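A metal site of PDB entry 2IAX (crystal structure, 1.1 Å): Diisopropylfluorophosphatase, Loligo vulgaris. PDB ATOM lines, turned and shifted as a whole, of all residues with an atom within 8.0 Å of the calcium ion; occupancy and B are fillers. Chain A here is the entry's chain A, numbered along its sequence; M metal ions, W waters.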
ATOM      1  N   GLY A  17     -23.825 -19.487  -0.874  1.00  0.00           N
ATOM      2  CA  GLY A  17     -23.344 -19.071  -2.189  1.00  0.00           C
ATOM      3  C   GLY A  17     -24.342 -18.287  -2.974  1.00  0.00           C
ATOM      4  O   GLY A  17     -24.243 -18.262  -4.179  1.00  0.00           O
ATOM      5  N   ALA A  18     -25.283 -17.626  -2.272  1.00  0.00           N
ATOM      6  CA  ALA A  18     -26.375 -16.859  -2.905  1.00  0.00           C
ATOM      7  C   ALA A  18     -25.932 -16.243  -4.233  1.00  0.00           C
ATOM      8  O   ALA A  18     -24.980 -15.432  -4.293  1.00  0.00           O
ATOM      9  CB  ALA A  18     -26.820 -15.768  -1.921  1.00  0.00           C
ATOM     10  N   GLU A  19     -26.707 -16.513  -5.254  1.00  0.00           N
ATOM     11  CA  GLU A  19     -26.319 -16.195  -6.622  1.00  0.00           C
ATOM     12  C   GLU A  19     -27.561 -16.047  -7.469  1.00  0.00           C
ATOM     13  O   GLU A  19     -28.722 -16.287  -7.009  1.00  0.00           O
ATOM     14  CB  GLU A  19     -25.416 -17.335  -7.218  1.00  0.00           C
ATOM     15  CG  GLU A  19     -23.922 -16.939  -7.288  1.00  0.00           C
ATOM     16  CD  GLU A  19     -23.555 -16.089  -8.483  1.00  0.00           C
ATOM     17  OE1 GLU A  19     -24.455 -15.471  -9.084  1.00  0.00           O
ATOM     18  OE2 GLU A  19     -22.364 -16.137  -8.903  1.00  0.00           O
ATOM     19  N   GLY A  20     -27.340 -15.707  -8.741  1.00  0.00           N
ATOM     20  CA  GLY A  20     -28.384 -15.743  -9.750  1.00  0.00           C
ATOM     21  C   GLY A  20     -29.703 -15.035  -9.439  1.00  0.00           C
ATOM     22  O   GLY A  20     -30.762 -15.651  -9.743  1.00  0.00           O
ATOM     23  N   PRO A  34     -26.002 -22.247  -4.926  1.00  0.00           N
ATOM     24  CA  PRO A  34     -25.145 -23.258  -5.512  1.00  0.00           C
ATOM     25  C   PRO A  34     -24.447 -24.095  -4.512  1.00  0.00           C
ATOM     26  O   PRO A  34     -24.097 -25.252  -4.860  1.00  0.00           O
ATOM     27  CB  PRO A  34     -24.140 -22.438  -6.352  1.00  0.00           C
ATOM     28  CG  PRO A  34     -24.274 -21.027  -5.875  1.00  0.00           C
ATOM     29  CD  PRO A  34     -25.689 -20.892  -5.431  1.00  0.00           C
ATOM     30  N   ALA A  72     -25.898 -21.765 -10.392  1.00  0.00           N
ATOM     31  CA  ALA A  72     -25.135 -20.567 -10.093  1.00  0.00           C
ATOM     32  C   ALA A  72     -25.573 -19.302 -10.806  1.00  0.00           C
ATOM     33  O   ALA A  72     -25.176 -18.188 -10.390  1.00  0.00           O
ATOM     34  CB  ALA A  72     -23.658 -20.798 -10.427  1.00  0.00           C
ATOM     35  N   GLY A  73     -26.365 -19.383 -11.839  1.00  0.00           N
ATOM     36  CA  GLY A  73     -26.736 -18.185 -12.573  1.00  0.00           C
ATOM     37  C   GLY A  73     -28.062 -18.429 -13.237  1.00  0.00           C
ATOM     38  O   GLY A  73     -28.406 -19.596 -13.536  1.00  0.00           O
ATOM     39  N   MET A  88     -22.860 -25.439 -12.370  1.00  0.00           N
ATOM     40  CA  MET A  88     -21.441 -25.808 -12.401  1.00  0.00           C
ATOM     41  C   MET A  88     -21.181 -27.313 -12.510  1.00  0.00           C
ATOM     42  O   MET A  88     -20.088 -27.736 -12.881  1.00  0.00           O
ATOM     43  CB  MET A  88     -20.674 -25.239 -11.223  1.00  0.00           C
ATOM     44  CG  MET A  88     -20.649 -23.693 -11.191  1.00  0.00           C
ATOM     45  SD  MET A  88     -19.375 -23.021 -12.258  1.00  0.00           S
ATOM     46  CE  MET A  88     -17.870 -23.317 -11.244  1.00  0.00           C
ATOM     47  N   CYS A 117     -21.402 -24.600 -16.054  1.00  0.00           N
ATOM     48  CA  CYS A 117     -21.645 -23.196 -16.358  1.00  0.00           C
ATOM     49  C   CYS A 117     -21.902 -22.382 -15.089  1.00  0.00           C
ATOM     50  O   CYS A 117     -22.295 -22.948 -14.038  1.00  0.00           O
ATOM     51  CB  CYS A 117     -22.832 -23.080 -17.318  1.00  0.00           C
ATOM     52  SG  CYS A 117     -22.503 -23.846 -18.937  1.00  0.00           S
ATOM     53  N   ASN A 118     -21.688 -21.059 -15.188  1.00  0.00           N
ATOM     54  CA  ASN A 118     -21.820 -20.184 -14.042  1.00  0.00           C
ATOM     55  C   ASN A 118     -22.816 -19.066 -14.236  1.00  0.00           C
ATOM     56  O   ASN A 118     -23.603 -18.819 -13.293  1.00  0.00           O
ATOM     57  CB  ASN A 118     -20.451 -19.603 -13.639  1.00  0.00           C
ATOM     58  CG  ASN A 118     -20.502 -18.955 -12.268  1.00  0.00           C
ATOM     59  OD1 ASN A 118     -20.937 -17.789 -12.132  1.00  0.00           O
ATOM     60  ND2 ASN A 118     -20.116 -19.717 -11.225  1.00  0.00           N
ATOM     61  N   ASP A 119     -22.813 -18.396 -15.385  1.00  0.00           N
ATOM     62  CA  ASP A 119     -23.774 -17.299 -15.566  1.00  0.00           C
ATOM     63  C   ASP A 119     -24.180 -17.247 -17.043  1.00  0.00           C
ATOM     64  O   ASP A 119     -23.557 -17.927 -17.890  1.00  0.00           O
ATOM     65  CB  ASP A 119     -23.168 -15.959 -15.081  1.00  0.00           C
ATOM     66  CG  ASP A 119     -24.182 -14.967 -14.618  1.00  0.00           C
ATOM     67  OD1 ASP A 119     -25.405 -15.155 -14.848  1.00  0.00           O
ATOM     68  OD2 ASP A 119     -23.797 -13.937 -14.005  1.00  0.00           O
ATOM     69  N   CYS A 120     -25.252 -16.522 -17.322  1.00  0.00           N
ATOM     70  CA  CYS A 120     -25.766 -16.448 -18.651  1.00  0.00           C
ATOM     71  C   CYS A 120     -26.514 -15.129 -18.869  1.00  0.00           C
ATOM     72  O   CYS A 120     -26.947 -14.484 -17.922  1.00  0.00           O
ATOM     73  CB  CYS A 120     -26.647 -17.676 -18.976  1.00  0.00           C
ATOM     74  SG  CYS A 120     -28.090 -17.928 -18.000  1.00  0.00           S
ATOM     75  N   THR A 131     -21.238 -18.424 -19.611  1.00  0.00           N
ATOM     76  CA  THR A 131     -19.867 -18.679 -19.154  1.00  0.00           C
ATOM     77  C   THR A 131     -19.794 -20.082 -18.525  1.00  0.00           C
ATOM     78  O   THR A 131     -20.719 -20.562 -17.838  1.00  0.00           O
ATOM     79  CB  THR A 131     -19.413 -17.661 -18.122  1.00  0.00           C
ATOM     80  OG1 THR A 131     -20.307 -17.689 -17.001  1.00  0.00           O
ATOM     81  CG2 THR A 131     -19.328 -16.262 -18.758  1.00  0.00           C
ATOM     82  N   PRO A 133     -16.933 -21.817 -16.434  1.00  0.00           N
ATOM     83  CA  PRO A 133     -15.624 -21.881 -15.760  1.00  0.00           C
ATOM     84  C   PRO A 133     -15.322 -23.227 -15.155  1.00  0.00           C
ATOM     85  O   PRO A 133     -14.175 -23.412 -14.734  1.00  0.00           O
ATOM     86  CB  PRO A 133     -15.767 -20.839 -14.660  1.00  0.00           C
ATOM     87  CG  PRO A 133     -17.225 -20.836 -14.330  1.00  0.00           C
ATOM     88  CD  PRO A 133     -17.962 -21.062 -15.653  1.00  0.00           C
ATOM     89  N   PHE A 171     -11.521 -18.677 -15.245  1.00  0.00           N
ATOM     90  CA  PHE A 171     -12.765 -18.442 -14.490  1.00  0.00           C
ATOM     91  C   PHE A 171     -13.607 -17.308 -15.127  1.00  0.00           C
ATOM     92  O   PHE A 171     -13.862 -16.278 -14.518  1.00  0.00           O
ATOM     93  CB  PHE A 171     -12.558 -18.259 -12.993  1.00  0.00           C
ATOM     94  CG  PHE A 171     -13.691 -18.800 -12.210  1.00  0.00           C
ATOM     95  CD1 PHE A 171     -14.846 -18.073 -12.044  1.00  0.00           C
ATOM     96  CD2 PHE A 171     -13.646 -20.111 -11.728  1.00  0.00           C
ATOM     97  CE1 PHE A 171     -15.966 -18.622 -11.376  1.00  0.00           C
ATOM     98  CE2 PHE A 171     -14.740 -20.652 -11.051  1.00  0.00           C
ATOM     99  CZ  PHE A 171     -15.882 -19.926 -10.866  1.00  0.00           C
ATOM    100  N   PRO A 172     -14.122 -17.574 -16.325  1.00  0.00           N
ATOM    101  CA  PRO A 172     -15.117 -16.675 -16.886  1.00  0.00           C
ATOM    102  C   PRO A 172     -16.372 -16.729 -15.985  1.00  0.00           C
ATOM    103  O   PRO A 172     -16.743 -17.822 -15.507  1.00  0.00           O
ATOM    104  CB  PRO A 172     -15.399 -17.295 -18.272  1.00  0.00           C
ATOM    105  CG  PRO A 172     -15.101 -18.746 -18.077  1.00  0.00           C
ATOM    106  CD  PRO A 172     -13.960 -18.808 -17.094  1.00  0.00           C
ATOM    107  N   ASN A 173     -17.015 -15.583 -15.757  1.00  0.00           N
ATOM    108  CA  ASN A 173     -17.959 -15.500 -14.651  1.00  0.00           C
ATOM    109  C   ASN A 173     -19.179 -14.739 -15.088  1.00  0.00           C
ATOM    110  O   ASN A 173     -19.991 -15.266 -15.848  1.00  0.00           O
ATOM    111  CB  ASN A 173     -17.212 -14.985 -13.410  1.00  0.00           C
ATOM    112  CG  ASN A 173     -17.953 -15.302 -12.137  1.00  0.00           C
ATOM    113  OD1 ASN A 173     -19.179 -15.559 -12.204  1.00  0.00           O
ATOM    114  ND2 ASN A 173     -17.305 -15.302 -11.010  1.00  0.00           N
ATOM    115  N   GLY A 174     -19.316 -13.452 -14.761  1.00  0.00           N
ATOM    116  CA  GLY A 174     -20.435 -12.671 -15.273  1.00  0.00           C
ATOM    117  C   GLY A 174     -20.330 -12.466 -16.760  1.00  0.00           C
ATOM    118  O   GLY A 174     -19.243 -12.574 -17.405  1.00  0.00           O
ATOM    119  N   ILE A 175     -21.490 -12.146 -17.347  1.00  0.00           N
ATOM    120  CA  ILE A 175     -21.589 -11.967 -18.782  1.00  0.00           C
ATOM    121  C   ILE A 175     -22.773 -11.070 -19.048  1.00  0.00           C
ATOM    122  O   ILE A 175     -23.790 -11.110 -18.308  1.00  0.00           O
ATOM    123  CB  ILE A 175     -21.688 -13.360 -19.485  1.00  0.00           C
ATOM    124  CG1 ILE A 175     -21.660 -13.242 -21.034  1.00  0.00           C
ATOM    125  CG2 ILE A 175     -22.913 -14.153 -18.993  1.00  0.00           C
ATOM    126  CD1 ILE A 175     -21.282 -14.594 -21.678  1.00  0.00           C
ATOM    127  N   ALA A 191     -16.720 -11.291 -17.742  1.00  0.00           N
ATOM    128  CA  ALA A 191     -15.816 -11.127 -16.639  1.00  0.00           C
ATOM    129  C   ALA A 191     -14.865 -12.320 -16.548  1.00  0.00           C
ATOM    130  O   ALA A 191     -15.304 -13.497 -16.689  1.00  0.00           O
ATOM    131  CB  ALA A 191     -16.617 -11.083 -15.340  1.00  0.00           C
ATOM    132  N   THR A 193     -12.618 -13.652 -13.572  1.00  0.00           N
ATOM    133  CA  THR A 193     -12.554 -13.174 -12.184  1.00  0.00           C
ATOM    134  C   THR A 193     -11.149 -12.830 -11.679  1.00  0.00           C
ATOM    135  O   THR A 193     -10.843 -11.712 -11.341  1.00  0.00           O
ATOM    136  CB  THR A 193     -13.316 -14.129 -11.276  1.00  0.00           C
ATOM    137  OG1 THR A 193     -14.700 -14.163 -11.698  1.00  0.00           O
ATOM    138  CG2 THR A 193     -13.292 -13.667  -9.842  1.00  0.00           C
ATOM    139  N   ALA A 226     -14.238  -9.490 -10.645  1.00  0.00           N
ATOM    140  CA  ALA A 226     -15.603  -9.387 -11.200  1.00  0.00           C
ATOM    141  C   ALA A 226     -16.338 -10.705 -11.143  1.00  0.00           C
ATOM    142  O   ALA A 226     -15.814 -11.713 -11.618  1.00  0.00           O
ATOM    143  CB  ALA A 226     -15.567  -8.885 -12.631  1.00  0.00           C
ATOM    144  N   ASP A 227     -17.578 -10.663 -10.595  1.00  0.00           N
ATOM    145  CA  ASP A 227     -18.460 -11.813 -10.524  1.00  0.00           C
ATOM    146  C   ASP A 227     -19.611 -11.510 -11.455  1.00  0.00           C
ATOM    147  O   ASP A 227     -19.429 -11.525 -12.694  1.00  0.00           O
ATOM    148  CB  ASP A 227     -18.765 -12.140  -9.073  1.00  0.00           C
ATOM    149  CG  ASP A 227     -19.528 -13.418  -8.895  1.00  0.00           C
ATOM    150  OD1 ASP A 227     -20.074 -13.962  -9.884  1.00  0.00           O
ATOM    151  OD2 ASP A 227     -19.572 -13.897  -7.730  1.00  0.00           O
ATOM    152  N   GLY A 228     -20.782 -11.094 -10.958  1.00  0.00           N
ATOM    153  CA  GLY A 228     -21.916 -10.814 -11.842  1.00  0.00           C
ATOM    154  C   GLY A 228     -21.967  -9.383 -12.281  1.00  0.00           C
ATOM    155  O   GLY A 228     -21.338  -8.468 -11.733  1.00  0.00           O
ATOM    156  N   MET A 229     -22.741  -9.163 -13.330  1.00  0.00           N
ATOM    157  CA  MET A 229     -22.847  -7.813 -13.914  1.00  0.00           C
ATOM    158  C   MET A 229     -24.234  -7.583 -14.485  1.00  0.00           C
ATOM    159  O   MET A 229     -24.933  -8.533 -14.904  1.00  0.00           O
ATOM    160  CB  MET A 229     -21.845  -7.653 -15.072  1.00  0.00           C
ATOM    161  CG  MET A 229     -21.984  -8.553 -16.208  1.00  0.00           C
ATOM    162  SD  MET A 229     -20.774  -8.406 -17.513  1.00  0.00           S
ATOM    163  CE  MET A 229     -19.347  -8.073 -16.279  1.00  0.00           C
ATOM    164  N   TRP A 242     -16.199  -9.045  -6.265  1.00  0.00           N
ATOM    165  CA  TRP A 242     -16.206  -9.933  -5.104  1.00  0.00           C
ATOM    166  C   TRP A 242     -14.869  -9.830  -4.391  1.00  0.00           C
ATOM    167  O   TRP A 242     -13.803  -9.994  -5.019  1.00  0.00           O
ATOM    168  CB  TRP A 242     -16.445 -11.339  -5.620  1.00  0.00           C
ATOM    169  CG  TRP A 242     -16.716 -12.417  -4.623  1.00  0.00           C
ATOM    170  CD1 TRP A 242     -17.932 -13.027  -4.448  1.00  0.00           C
ATOM    171  CD2 TRP A 242     -15.776 -13.170  -3.836  1.00  0.00           C
ATOM    172  NE1 TRP A 242     -17.817 -14.052  -3.547  1.00  0.00           N
ATOM    173  CE2 TRP A 242     -16.508 -14.195  -3.187  1.00  0.00           C
ATOM    174  CE3 TRP A 242     -14.387 -13.073  -3.602  1.00  0.00           C
ATOM    175  CZ2 TRP A 242     -15.914 -15.135  -2.328  1.00  0.00           C
ATOM    176  CZ3 TRP A 242     -13.786 -13.992  -2.735  1.00  0.00           C
ATOM    177  CH2 TRP A 242     -14.542 -15.030  -2.136  1.00  0.00           C
ATOM    178  N   SER A 269     -21.744 -10.763  -5.044  1.00  0.00           N
ATOM    179  CA  SER A 269     -21.597 -11.796  -6.044  1.00  0.00           C
ATOM    180  C   SER A 269     -22.394 -11.513  -7.300  1.00  0.00           C
ATOM    181  O   SER A 269     -21.848 -11.615  -8.403  1.00  0.00           O
ATOM    182  CB  SER A 269     -22.013 -13.115  -5.454  1.00  0.00           C
ATOM    183  OG  SER A 269     -23.403 -13.137  -5.211  1.00  0.00           O
ATOM    184  N   ASN A 270     -23.639 -11.104  -7.231  1.00  0.00           N
ATOM    185  CA  ASN A 270     -24.405 -10.911  -8.420  1.00  0.00           C
ATOM    186  C   ASN A 270     -25.491  -9.887  -8.148  1.00  0.00           C
ATOM    187  O   ASN A 270     -25.759  -9.500  -6.977  1.00  0.00           O
ATOM    188  CB  ASN A 270     -24.949 -12.247  -8.951  1.00  0.00           C
ATOM    189  CG  ASN A 270     -25.005 -12.304 -10.486  1.00  0.00           C
ATOM    190  OD1 ASN A 270     -24.801 -13.423 -11.073  1.00  0.00           O
ATOM    191  ND2 ASN A 270     -25.206 -11.227 -11.130  1.00  0.00           N
ATOM    192  N   THR A 283     -26.827 -10.255  -4.358  1.00  0.00           N
ATOM    193  CA  THR A 283     -26.452 -11.394  -3.537  1.00  0.00           C
ATOM    194  C   THR A 283     -24.997 -11.234  -3.069  1.00  0.00           C
ATOM    195  O   THR A 283     -24.195 -10.565  -3.703  1.00  0.00           O
ATOM    196  CB  THR A 283     -26.622 -12.689  -4.322  1.00  0.00           C
ATOM    197  OG1 THR A 283     -25.830 -12.598  -5.565  1.00  0.00           O
ATOM    198  CG2 THR A 283     -28.012 -12.925  -4.783  1.00  0.00           C
ATOM    199  N   HIS A 285     -21.667 -13.062  -0.488  1.00  0.00           N
ATOM    200  CA  HIS A 285     -21.127 -14.271   0.123  1.00  0.00           C
ATOM    201  C   HIS A 285     -20.399 -14.034   1.464  1.00  0.00           C
ATOM    202  O   HIS A 285     -19.792 -15.011   1.943  1.00  0.00           O
ATOM    203  CB  HIS A 285     -20.215 -15.022  -0.821  1.00  0.00           C
ATOM    204  CG  HIS A 285     -20.899 -15.440  -2.077  1.00  0.00           C
ATOM    205  ND1 HIS A 285     -20.230 -15.881  -3.210  1.00  0.00           N
ATOM    206  CD2 HIS A 285     -22.217 -15.486  -2.382  1.00  0.00           C
ATOM    207  CE1 HIS A 285     -21.105 -16.129  -4.160  1.00  0.00           C
ATOM    208  NE2 HIS A 285     -22.319 -15.888  -3.693  1.00  0.00           N
HETATM  209 CA    CA M   1     -21.159 -15.836 -10.855  1.00  0.00          CA
HETATM  210  O   HOH W   1     -23.405 -16.449 -11.696  1.00  0.00           O
HETATM  211  O   HOH W   2     -21.668 -14.141 -12.388  1.00  0.00           O
HETATM  212  O   HOH W   3     -19.506 -16.488  -9.229  1.00  0.00           O
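Water W3 lies within hydrogen-bond range of the side-chain carboxylate (OD2) of Asp 227 (3.0 Å) and the side-chain amide nitrogen (ND2) of Asn 173 (3.1 Å).
The side-chain hydroxyl of Thr 131 lies within hydrogen-bond range of the backbone carbonyl oxygen of Asn 173 (2.7 Å).
The backbone carbonyl oxygen of Thr 131 is in hydrogen-bond range of the backbone NH of Asn 118, 2.9 Å away.
OD1 of Asn 270 sits close to OE1 of Glu 19 (2.9 Å).
N of Gly 174 lies within hydrogen-bond range of O of Asp 227 (2.8 Å).
N of Gly 73 is in hydrogen-bond range of O of Asn 118 (3.2 Å).
The side-chain amide nitrogen (ND2) of Asn 173 sits at hydrogen-bond distance from the side-chain hydroxyl (OG1) of Thr 193 (2.9 Å).
O of Ala 191 sits at hydrogen-bond distance from N of Asn 173.
The side-chain sulfur (SD) of Met 88 lies within hydrogen-bond range of the side-chain amide nitrogen (ND2) of Asn 118.
Four residues have an atom within 4 Å of the calcium ion: Glu 19, Asn 118, Asn 173 and Asp 227.
The nearest printed residue that does not touch the calcium ion is Asn 270 (4.4 Å).
The calcium ion is bound by OE2 of Glu 19, water W2, OD1 of Asn 118, OD1 of Asp 227, water W3, OD1 of Asn 173 and water W1.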
